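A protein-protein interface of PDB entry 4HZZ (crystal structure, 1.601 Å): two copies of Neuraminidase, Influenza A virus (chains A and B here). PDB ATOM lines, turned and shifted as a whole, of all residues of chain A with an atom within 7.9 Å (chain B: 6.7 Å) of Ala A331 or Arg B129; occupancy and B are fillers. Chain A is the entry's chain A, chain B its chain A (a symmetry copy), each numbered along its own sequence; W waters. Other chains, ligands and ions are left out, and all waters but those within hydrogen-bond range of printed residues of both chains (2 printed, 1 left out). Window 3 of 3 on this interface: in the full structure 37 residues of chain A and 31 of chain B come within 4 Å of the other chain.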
ATOM      1  N   LEU A   7      -7.301 -17.018  12.752  1.00  0.00           N
ATOM      2  CA  LEU A   7      -6.544 -16.790  11.522  1.00  0.00           C
ATOM      3  C   LEU A   7      -7.380 -17.103  10.288  1.00  0.00           C
ATOM      4  O   LEU A   7      -8.283 -17.939  10.349  1.00  0.00           O
ATOM      5  CB  LEU A   7      -5.294 -17.676  11.517  1.00  0.00           C
ATOM      6  CG  LEU A   7      -4.414 -17.623  12.765  1.00  0.00           C
ATOM      7  CD1 LEU A   7      -3.291 -18.646  12.659  1.00  0.00           C
ATOM      8  CD2 LEU A   7      -3.835 -16.234  12.965  1.00  0.00           C
ATOM      9  N   PRO A   8      -7.078 -16.445   9.156  1.00  0.00           N
ATOM     10  CA  PRO A   8      -7.697 -16.761   7.863  1.00  0.00           C
ATOM     11  C   PRO A   8      -7.128 -18.046   7.296  1.00  0.00           C
ATOM     12  O   PRO A   8      -6.056 -18.479   7.718  1.00  0.00           O
ATOM     13  CB  PRO A   8      -7.227 -15.606   6.969  1.00  0.00           C
ATOM     14  CG  PRO A   8      -5.891 -15.250   7.534  1.00  0.00           C
ATOM     15  CD  PRO A   8      -6.087 -15.356   9.033  1.00  0.00           C
ATOM     16  N   CYS A  10      -5.109 -20.087   4.564  1.00  0.00           N
ATOM     17  CA  CYS A  10      -4.011 -19.812   3.645  1.00  0.00           C
ATOM     18  C   CYS A  10      -4.520 -19.915   2.217  1.00  0.00           C
ATOM     19  O   CYS A  10      -5.530 -20.558   1.956  1.00  0.00           O
ATOM     20  CB  CYS A  10      -2.893 -20.850   3.832  1.00  0.00           C
ATOM     21  SG  CYS A  10      -2.204 -21.009   5.502  1.00  0.00           S
ATOM     22  N   PHE A  18      -1.279 -36.599   1.591  1.00  0.00           N
ATOM     23  CA  PHE A  18      -0.528 -36.332   2.822  1.00  0.00           C
ATOM     24  C   PHE A  18      -0.169 -37.656   3.515  1.00  0.00           C
ATOM     25  O   PHE A  18       0.918 -38.191   3.300  1.00  0.00           O
ATOM     26  CB  PHE A  18      -1.426 -35.450   3.705  1.00  0.00           C
ATOM     27  CG  PHE A  18      -0.755 -34.813   4.908  1.00  0.00           C
ATOM     28  CD1 PHE A  18       0.604 -34.566   4.961  1.00  0.00           C
ATOM     29  CD2 PHE A  18      -1.543 -34.400   5.986  1.00  0.00           C
ATOM     30  CE1 PHE A  18       1.183 -33.936   6.089  1.00  0.00           C
ATOM     31  CE2 PHE A  18      -0.979 -33.771   7.092  1.00  0.00           C
ATOM     32  CZ  PHE A  18       0.388 -33.549   7.144  1.00  0.00           C
ATOM     33  N   HIS A  19      -1.091 -38.186   4.321  1.00  0.00           N
ATOM     34  CA  HIS A  19      -0.886 -39.437   5.061  1.00  0.00           C
ATOM     35  C   HIS A  19      -1.933 -40.473   4.648  1.00  0.00           C
ATOM     36  O   HIS A  19      -3.082 -40.115   4.361  1.00  0.00           O
ATOM     37  CB  HIS A  19      -1.050 -39.197   6.572  1.00  0.00           C
ATOM     38  CG  HIS A  19       0.053 -38.399   7.202  1.00  0.00           C
ATOM     39  ND1 HIS A  19       1.239 -38.961   7.631  1.00  0.00           N
ATOM     40  CD2 HIS A  19       0.123 -37.086   7.528  1.00  0.00           C
ATOM     41  CE1 HIS A  19       2.004 -38.020   8.156  1.00  0.00           C
ATOM     42  NE2 HIS A  19       1.351 -36.870   8.101  1.00  0.00           N
ATOM     43  N   ASP A  45       2.446 -30.008  18.181  1.00  0.00           N
ATOM     44  CA  ASP A  45       3.577 -30.896  17.907  1.00  0.00           C
ATOM     45  C   ASP A  45       3.274 -31.955  16.844  1.00  0.00           C
ATOM     46  O   ASP A  45       4.177 -32.425  16.156  1.00  0.00           O
ATOM     47  CB  ASP A  45       4.004 -31.606  19.191  1.00  0.00           C
ATOM     48  CG  ASP A  45       4.369 -30.640  20.295  1.00  0.00           C
ATOM     49  OD1 ASP A  45       5.129 -29.693  20.016  1.00  0.00           O
ATOM     50  OD2 ASP A  45       3.887 -30.829  21.431  1.00  0.00           O
ATOM     51  N   CYS A  47      -0.006 -33.966  14.188  1.00  0.00           N
ATOM     52  CA  CYS A  47      -1.370 -34.292  13.787  1.00  0.00           C
ATOM     53  C   CYS A  47      -1.657 -35.719  14.198  1.00  0.00           C
ATOM     54  O   CYS A  47      -0.757 -36.553  14.232  1.00  0.00           O
ATOM     55  CB  CYS A  47      -1.549 -34.146  12.286  1.00  0.00           C
ATOM     56  SG  CYS A  47      -1.616 -32.403  11.758  1.00  0.00           S
ATOM     57  N   ILE A 328      -7.714 -28.351  10.082  1.00  0.00           N
ATOM     58  CA  ILE A 328      -6.769 -27.286   9.763  1.00  0.00           C
ATOM     59  C   ILE A 328      -5.407 -27.514  10.400  1.00  0.00           C
ATOM     60  O   ILE A 328      -5.278 -28.158  11.447  1.00  0.00           O
ATOM     61  CB  ILE A 328      -7.279 -25.901  10.193  1.00  0.00           C
ATOM     62  CG1 ILE A 328      -7.695 -25.909  11.666  1.00  0.00           C
ATOM     63  CG2 ILE A 328      -8.422 -25.440   9.294  1.00  0.00           C
ATOM     64  CD1 ILE A 328      -8.138 -24.533  12.178  1.00  0.00           C
ATOM     65  N   VAL A 329      -4.382 -26.968   9.755  1.00  0.00           N
ATOM     66  CA  VAL A 329      -3.033 -27.014  10.291  1.00  0.00           C
ATOM     67  C   VAL A 329      -2.484 -25.600  10.297  1.00  0.00           C
ATOM     68  O   VAL A 329      -2.490 -24.928   9.268  1.00  0.00           O
ATOM     69  CB  VAL A 329      -2.120 -27.911   9.441  1.00  0.00           C
ATOM     70  CG1 VAL A 329      -0.748 -27.990  10.074  1.00  0.00           C
ATOM     71  CG2 VAL A 329      -2.719 -29.299   9.336  1.00  0.00           C
ATOM     72  N   LYS A 330      -2.041 -25.126  11.456  1.00  0.00           N
ATOM     73  CA  LYS A 330      -1.529 -23.760  11.529  1.00  0.00           C
ATOM     74  C   LYS A 330      -0.241 -23.611  10.736  1.00  0.00           C
ATOM     75  O   LYS A 330       0.681 -24.416  10.886  1.00  0.00           O
ATOM     76  CB  LYS A 330      -1.284 -23.350  12.982  1.00  0.00           C
ATOM     77  CG  LYS A 330      -0.806 -21.910  13.117  1.00  0.00           C
ATOM     78  CD  LYS A 330      -0.584 -21.509  14.560  1.00  0.00           C
ATOM     79  CE  LYS A 330       0.079 -20.140  14.634  1.00  0.00           C
ATOM     80  NZ  LYS A 330       0.428 -19.759  16.029  1.00  0.00           N
ATOM     81  N   ALA A 331      -0.196 -22.567   9.909  1.00  0.00           N
ATOM     82  CA  ALA A 331       0.935 -22.251   9.044  1.00  0.00           C
ATOM     83  C   ALA A 331       1.730 -21.333   9.971  1.00  0.00           C
ATOM     84  O   ALA A 331       2.286 -21.792  10.968  1.00  0.00           O
ATOM     85  CB  ALA A 331       0.561 -22.511   7.608  1.00  0.00           C
ATOM     86  N   LYS A 332       1.784 -20.049   9.651  1.00  0.00           N
ATOM     87  CA  LYS A 332       2.528 -19.090  10.469  1.00  0.00           C
ATOM     88  C   LYS A 332       1.363 -18.166  10.845  1.00  0.00           C
ATOM     89  O   LYS A 332       0.977 -18.095  12.014  1.00  0.00           O
ATOM     90  CB  LYS A 332       3.274 -18.530   9.255  1.00  0.00           C
ATOM     91  CG  LYS A 332       4.553 -19.270   8.907  1.00  0.00           C
ATOM     92  CD  LYS A 332       5.562 -19.207  10.039  1.00  0.00           C
ATOM     93  CE  LYS A 332       6.884 -19.845   9.628  1.00  0.00           C
ATOM     94  NZ  LYS A 332       7.905 -19.774  10.711  1.00  0.00           N
ATOM     95  N   ASP A 333       0.806 -17.473   9.855  1.00  0.00           N
ATOM     96  CA  ASP A 333      -0.248 -16.488  10.103  1.00  0.00           C
ATOM     97  C   ASP A 333      -1.577 -16.861   9.442  1.00  0.00           C
ATOM     98  O   ASP A 333      -2.478 -16.025   9.307  1.00  0.00           O
ATOM     99  CB  ASP A 333       0.199 -15.104   9.626  1.00  0.00           C
ATOM    100  CG  ASP A 333       1.437 -14.607  10.350  1.00  0.00           C
ATOM    101  OD1 ASP A 333       1.584 -14.898  11.557  1.00  0.00           O
ATOM    102  OD2 ASP A 333       2.260 -13.919   9.711  1.00  0.00           O
ATOM    103  N   CYS A 334      -1.697 -18.119   9.031  1.00  0.00           N
ATOM    104  CA  CYS A 334      -2.929 -18.605   8.423  1.00  0.00           C
ATOM    105  C   CYS A 334      -3.090 -20.088   8.724  1.00  0.00           C
ATOM    106  O   CYS A 334      -2.142 -20.733   9.167  1.00  0.00           O
ATOM    107  CB  CYS A 334      -2.938 -18.365   6.908  1.00  0.00           C
ATOM    108  SG  CYS A 334      -1.549 -19.116   5.969  1.00  0.00           S
ATOM    109  N   PHE A 335      -4.291 -20.608   8.481  1.00  0.00           N
ATOM    110  CA  PHE A 335      -4.571 -22.038   8.619  1.00  0.00           C
ATOM    111  C   PHE A 335      -4.605 -22.721   7.264  1.00  0.00           C
ATOM    112  O   PHE A 335      -5.290 -22.284   6.348  1.00  0.00           O
ATOM    113  CB  PHE A 335      -5.923 -22.288   9.305  1.00  0.00           C
ATOM    114  CG  PHE A 335      -5.951 -21.935  10.757  1.00  0.00           C
ATOM    115  CD1 PHE A 335      -5.087 -22.550  11.645  1.00  0.00           C
ATOM    116  CD2 PHE A 335      -6.879 -21.023  11.247  1.00  0.00           C
ATOM    117  CE1 PHE A 335      -5.124 -22.243  13.006  1.00  0.00           C
ATOM    118  CE2 PHE A 335      -6.918 -20.714  12.604  1.00  0.00           C
ATOM    119  CZ  PHE A 335      -6.031 -21.320  13.477  1.00  0.00           C
ATOM    120  N   GLN A 336      -3.875 -23.821   7.144  1.00  0.00           N
ATOM    121  CA  GLN A 336      -3.904 -24.601   5.915  1.00  0.00           C
ATOM    122  C   GLN A 336      -5.104 -25.533   5.960  1.00  0.00           C
ATOM    123  O   GLN A 336      -5.303 -26.225   6.969  1.00  0.00           O
ATOM    124  CB  GLN A 336      -2.618 -25.419   5.825  1.00  0.00           C
ATOM    125  CG  GLN A 336      -2.577 -26.419   4.684  1.00  0.00           C
ATOM    126  CD  GLN A 336      -1.279 -27.197   4.699  1.00  0.00           C
ATOM    127  OE1 GLN A 336      -0.736 -27.485   5.772  1.00  0.00           O
ATOM    128  NE2 GLN A 336      -0.745 -27.499   3.516  1.00  0.00           N
ATOM    129  N   PRO A 337      -5.923 -25.538   4.891  1.00  0.00           N
ATOM    130  CA  PRO A 337      -7.085 -26.440   4.833  1.00  0.00           C
ATOM    131  C   PRO A 337      -6.686 -27.844   4.415  1.00  0.00           C
ATOM    132  O   PRO A 337      -6.000 -28.026   3.404  1.00  0.00           O
ATOM    133  CB  PRO A 337      -7.976 -25.794   3.757  1.00  0.00           C
ATOM    134  CG  PRO A 337      -6.972 -25.154   2.822  1.00  0.00           C
ATOM    135  CD  PRO A 337      -5.838 -24.666   3.702  1.00  0.00           C
ATOM    136  N   CYS A 338      -7.125 -28.830   5.190  1.00  0.00           N
ATOM    137  CA  CYS A 338      -6.849 -30.228   4.882  1.00  0.00           C
ATOM    138  C   CYS A 338      -8.131 -31.027   5.061  1.00  0.00           C
ATOM    139  O   CYS A 338      -9.123 -30.527   5.593  1.00  0.00           O
ATOM    140  CB  CYS A 338      -5.789 -30.795   5.832  1.00  0.00           C
ATOM    141  SG  CYS A 338      -4.158 -29.982   5.792  1.00  0.00           S
ATOM    142  N   CYS A 365      -3.942 -32.256   1.822  1.00  0.00           N
ATOM    143  CA  CYS A 365      -3.836 -30.867   2.273  1.00  0.00           C
ATOM    144  C   CYS A 365      -3.760 -29.909   1.103  1.00  0.00           C
ATOM    145  O   CYS A 365      -3.274 -30.251   0.030  1.00  0.00           O
ATOM    146  CB  CYS A 365      -2.631 -30.650   3.188  1.00  0.00           C
ATOM    147  SG  CYS A 365      -2.855 -31.288   4.876  1.00  0.00           S
ATOM    148  N   GLY A 366      -4.241 -28.692   1.330  1.00  0.00           N
ATOM    149  CA  GLY A 366      -4.251 -27.682   0.287  1.00  0.00           C
ATOM    150  C   GLY A 366      -2.970 -26.882   0.208  1.00  0.00           C
ATOM    151  O   GLY A 366      -2.421 -26.459   1.231  1.00  0.00           O
ATOM    152  N   LEU A 367      -2.499 -26.672  -1.018  1.00  0.00           N
ATOM    153  CA  LEU A 367      -1.359 -25.793  -1.278  1.00  0.00           C
ATOM    154  C   LEU A 367      -1.715 -24.849  -2.407  1.00  0.00           C
ATOM    155  O   LEU A 367      -2.581 -25.159  -3.230  1.00  0.00           O
ATOM    156  CB  LEU A 367      -0.123 -26.602  -1.697  1.00  0.00           C
ATOM    157  CG  LEU A 367       0.501 -27.569  -0.687  1.00  0.00           C
ATOM    158  CD1 LEU A 367       1.550 -28.416  -1.392  1.00  0.00           C
ATOM    159  CD2 LEU A 367       1.137 -26.814   0.475  1.00  0.00           C
ATOM    160  N   ILE B 124       6.358 -31.655  -0.138  1.00  0.00           N
ATOM    161  CA  ILE B 124       7.432 -31.266   0.762  1.00  0.00           C
ATOM    162  C   ILE B 124       6.836 -31.119   2.155  1.00  0.00           C
ATOM    163  O   ILE B 124       5.900 -30.340   2.357  1.00  0.00           O
ATOM    164  CB  ILE B 124       8.072 -29.917   0.355  1.00  0.00           C
ATOM    165  CG1 ILE B 124       8.503 -29.930  -1.115  1.00  0.00           C
ATOM    166  CG2 ILE B 124       9.234 -29.568   1.296  1.00  0.00           C
ATOM    167  CD1 ILE B 124       9.433 -31.080  -1.491  1.00  0.00           C
ATOM    168  N   ILE B 125       7.363 -31.893   3.098  1.00  0.00           N
ATOM    169  CA  ILE B 125       6.910 -31.861   4.486  1.00  0.00           C
ATOM    170  C   ILE B 125       8.011 -31.246   5.341  1.00  0.00           C
ATOM    171  O   ILE B 125       9.175 -31.619   5.220  1.00  0.00           O
ATOM    172  CB  ILE B 125       6.635 -33.286   5.021  1.00  0.00           C
ATOM    173  CG1 ILE B 125       5.840 -34.125   4.006  1.00  0.00           C
ATOM    174  CG2 ILE B 125       6.000 -33.232   6.413  1.00  0.00           C
ATOM    175  CD1 ILE B 125       4.486 -33.579   3.660  1.00  0.00           C
ATOM    176  N   TYR B 126       7.650 -30.296   6.196  1.00  0.00           N
ATOM    177  CA  TYR B 126       8.633 -29.633   7.035  1.00  0.00           C
ATOM    178  C   TYR B 126       8.024 -29.432   8.414  1.00  0.00           C
ATOM    179  O   TYR B 126       6.962 -28.831   8.543  1.00  0.00           O
ATOM    180  CB  TYR B 126       9.061 -28.290   6.423  1.00  0.00           C
ATOM    181  CG  TYR B 126      10.169 -27.638   7.214  1.00  0.00           C
ATOM    182  CD1 TYR B 126      11.491 -28.040   7.060  1.00  0.00           C
ATOM    183  CD2 TYR B 126       9.894 -26.642   8.136  1.00  0.00           C
ATOM    184  CE1 TYR B 126      12.507 -27.456   7.793  1.00  0.00           C
ATOM    185  CE2 TYR B 126      10.901 -26.060   8.887  1.00  0.00           C
ATOM    186  CZ  TYR B 126      12.205 -26.463   8.706  1.00  0.00           C
ATOM    187  OH  TYR B 126      13.212 -25.883   9.446  1.00  0.00           O
ATOM    188  N   GLY B 127       8.686 -29.965   9.437  1.00  0.00           N
ATOM    189  CA  GLY B 127       8.138 -29.932  10.790  1.00  0.00           C
ATOM    190  C   GLY B 127       6.758 -30.579  10.858  1.00  0.00           C
ATOM    191  O   GLY B 127       5.907 -30.194  11.682  1.00  0.00           O
ATOM    192  N   GLY B 128       6.523 -31.563   9.994  1.00  0.00           N
ATOM    193  CA  GLY B 128       5.274 -32.303  10.020  1.00  0.00           C
ATOM    194  C   GLY B 128       4.154 -31.687   9.196  1.00  0.00           C
ATOM    195  O   GLY B 128       3.104 -32.302   9.031  1.00  0.00           O
ATOM    196  N   ARG B 129       4.367 -30.467   8.697  1.00  0.00           N
ATOM    197  CA  ARG B 129       3.353 -29.807   7.879  1.00  0.00           C
ATOM    198  C   ARG B 129       3.717 -29.880   6.408  1.00  0.00           C
ATOM    199  O   ARG B 129       4.884 -29.724   6.050  1.00  0.00           O
ATOM    200  CB  ARG B 129       3.214 -28.333   8.286  1.00  0.00           C
ATOM    201  CG  ARG B 129       2.096 -27.614   7.543  1.00  0.00           C
ATOM    202  CD  ARG B 129       1.853 -26.193   8.057  1.00  0.00           C
ATOM    203  NE  ARG B 129       2.694 -25.197   7.395  1.00  0.00           N
ATOM    204  CZ  ARG B 129       2.488 -24.748   6.157  1.00  0.00           C
ATOM    205  NH1 ARG B 129       1.483 -25.228   5.426  1.00  0.00           N
ATOM    206  NH2 ARG B 129       3.294 -23.827   5.639  1.00  0.00           N
ATOM    207  N   MET B 130       2.725 -30.099   5.547  1.00  0.00           N
ATOM    208  CA  MET B 130       2.994 -30.037   4.115  1.00  0.00           C
ATOM    209  C   MET B 130       3.112 -28.576   3.701  1.00  0.00           C
ATOM    210  O   MET B 130       2.140 -27.823   3.773  1.00  0.00           O
ATOM    211  CB  MET B 130       1.885 -30.719   3.321  1.00  0.00           C
ATOM    212  CG  MET B 130       2.168 -30.766   1.830  1.00  0.00           C
ATOM    213  SD  MET B 130       0.748 -31.313   0.856  1.00  0.00           S
ATOM    214  CE  MET B 130       0.487 -32.964   1.510  1.00  0.00           C
ATOM    215  N   THR B 131       4.300 -28.176   3.262  1.00  0.00           N
ATOM    216  CA  THR B 131       4.612 -26.761   3.054  1.00  0.00           C
ATOM    217  C   THR B 131       4.780 -26.353   1.589  1.00  0.00           C
ATOM    218  O   THR B 131       4.712 -25.165   1.262  1.00  0.00           O
ATOM    219  CB  THR B 131       5.914 -26.392   3.774  1.00  0.00           C
ATOM    220  OG1 THR B 131       6.926 -27.335   3.411  1.00  0.00           O
ATOM    221  CG2 THR B 131       5.734 -26.443   5.284  1.00  0.00           C
ATOM    222  N   ASP B 132       5.052 -27.312   0.712  1.00  0.00           N
ATOM    223  CA  ASP B 132       5.240 -26.994  -0.707  1.00  0.00           C
ATOM    224  C   ASP B 132       5.095 -28.271  -1.528  1.00  0.00           C
ATOM    225  O   ASP B 132       4.837 -29.343  -0.979  1.00  0.00           O
ATOM    226  CB  ASP B 132       6.623 -26.353  -0.923  1.00  0.00           C
ATOM    227  CG  ASP B 132       6.626 -25.273  -2.012  1.00  0.00           C
ATOM    228  OD1 ASP B 132       5.756 -25.303  -2.910  1.00  0.00           O
ATOM    229  OD2 ASP B 132       7.518 -24.390  -1.981  1.00  0.00           O
ATOM    230  N   GLU B 178      13.290 -24.085   5.073  1.00  0.00           N
ATOM    231  CA  GLU B 178      12.128 -24.190   5.953  1.00  0.00           C
ATOM    232  C   GLU B 178      10.881 -24.661   5.210  1.00  0.00           C
ATOM    233  O   GLU B 178       9.775 -24.155   5.434  1.00  0.00           O
ATOM    234  CB  GLU B 178      11.862 -22.870   6.677  1.00  0.00           C
ATOM    235  CG  GLU B 178      13.011 -22.440   7.571  1.00  0.00           C
ATOM    236  CD  GLU B 178      12.744 -21.112   8.245  1.00  0.00           C
ATOM    237  OE1 GLU B 178      11.574 -20.848   8.597  1.00  0.00           O
ATOM    238  OE2 GLU B 178      13.701 -20.335   8.420  1.00  0.00           O
ATOM    239  N   GLY B 179      11.067 -25.642   4.335  1.00  0.00           N
ATOM    240  CA  GLY B 179       9.952 -26.266   3.638  1.00  0.00           C
ATOM    241  C   GLY B 179       9.468 -25.533   2.399  1.00  0.00           C
ATOM    242  O   GLY B 179       8.555 -26.002   1.718  1.00  0.00           O
ATOM    243  N   LYS B 180      10.071 -24.382   2.104  1.00  0.00           N
ATOM    244  CA  LYS B 180       9.690 -23.620   0.916  1.00  0.00           C
ATOM    245  C   LYS B 180      10.750 -23.713  -0.183  1.00  0.00           C
ATOM    246  O   LYS B 180      11.925 -23.439   0.050  1.00  0.00           O
ATOM    247  CB  LYS B 180       9.451 -22.150   1.268  1.00  0.00           C
ATOM    248  CG  LYS B 180       8.235 -21.897   2.161  1.00  0.00           C
ATOM    249  CD  LYS B 180       7.015 -22.723   1.733  1.00  0.00           C
ATOM    250  CE  LYS B 180       5.809 -22.439   2.616  1.00  0.00           C
ATOM    251  NZ  LYS B 180       5.333 -21.028   2.470  1.00  0.00           N
HETATM  252  O   HOH W   1       2.695 -34.920   9.592  1.00  0.00           O
HETATM  253  O   HOH W   2       0.031 -30.045   6.451  1.00  0.00           O
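No position is printed for both chains.
Of the 10 pairs that touch across the chains among the printed residues, none has its exchanged pair printed and touching as well.
Water W1 bridges the backbone carbonyl oxygen (O) of Gly B128 (2.7 Å) and a ring nitrogen (NE2) of His A19 (2.8 Å).
Water W2 lies within hydrogen-bond range of OE1 of Gln A336 (2.8 Å), N of Met B130 (2.8 Å) and SG of Cys A365 (3.5 Å).
Printed residues of chain B within 4 Å of Phe A18: Gly B128 (3.5 Å) and Met B130 (3.8 Å).
Of the printed residues of chain B, Lys A330 touches Arg B129.
Of chain B, only Arg B129 (3.3 Å) comes within 4 Å of Ala A331.
Pro A337 touches none of the printed residues of chain B.
Of the printed residues of chain B, Leu A367 touches Met B130, Thr B131 and Asp B132.
Of chain A, only Phe A18 comes within 4 Å of Gly B128.
Arg B129 touches just these residues of chain A: Val A329 (3.8 Å), Lys A330 (3.5 Å), Ala A331 (3.3 Å) and Gln A336 (3.2 Å).
Gly B179 touches none of the printed residues of chain A.
The nearest printed residue of chain B that does not touch Gln A336 is Thr B131 (5.1 Å).
Hydrophobic or aromatic side chains of chain A within 4 Å of the printed part of chain B: Phe A18, Val A329, Ala A331 and Leu A367.
Among the printed residues, no Asp or Glu carboxylate lies within 4 Å of a Lys or Arg side-chain nitrogen of the other chain.
O of Gly B128 touches CZ of Phe A18, 3.5 Å away.
Phe A18 touches Met B130 (CA to CE, 3.8 Å).
Val A329 touches Arg B129.
CD of Arg B129 touches O of Lys A330 (3.5 Å).
Ala A331 touches Arg B129 (CB to CZ, 3.3 Å).
Leu A367 touches Met B130.
Thr B131 touches Leu A367 (C to CD2, 3.8 Å).
Asp B132 touches Leu A367.
NE2 of Gln A336 is in hydrogen-bond range of O of Met B130 (2.9 Å).
NH1 of Arg B129 sits at hydrogen-bond distance from OE1 of Gln A336.
OG1 of Thr B131 is in hydrogen-bond range of O of Gly B179, at 2.7 Å.
The backbone NH (N) of Gln A336 lies within hydrogen-bond range of the side-chain sulfur (SG) of Cys A10.
SG of Cys A10 is disulfide-bonded to SG of Cys A334, at 2.1 Å.
The side-chain amide nitrogen (NE2) of Gln A336 lies within hydrogen-bond range of the backbone carbonyl oxygen (O) of Gly A366, 3.0 Å away.
The side-chain sulfur of Cys A338 is disulfide-bonded to the side-chain sulfur of Cys A365.
The backbone NH (N) of Ile B124 lies within hydrogen-bond range of the backbone carbonyl oxygen (O) of Asp B132, at 2.9 Å.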
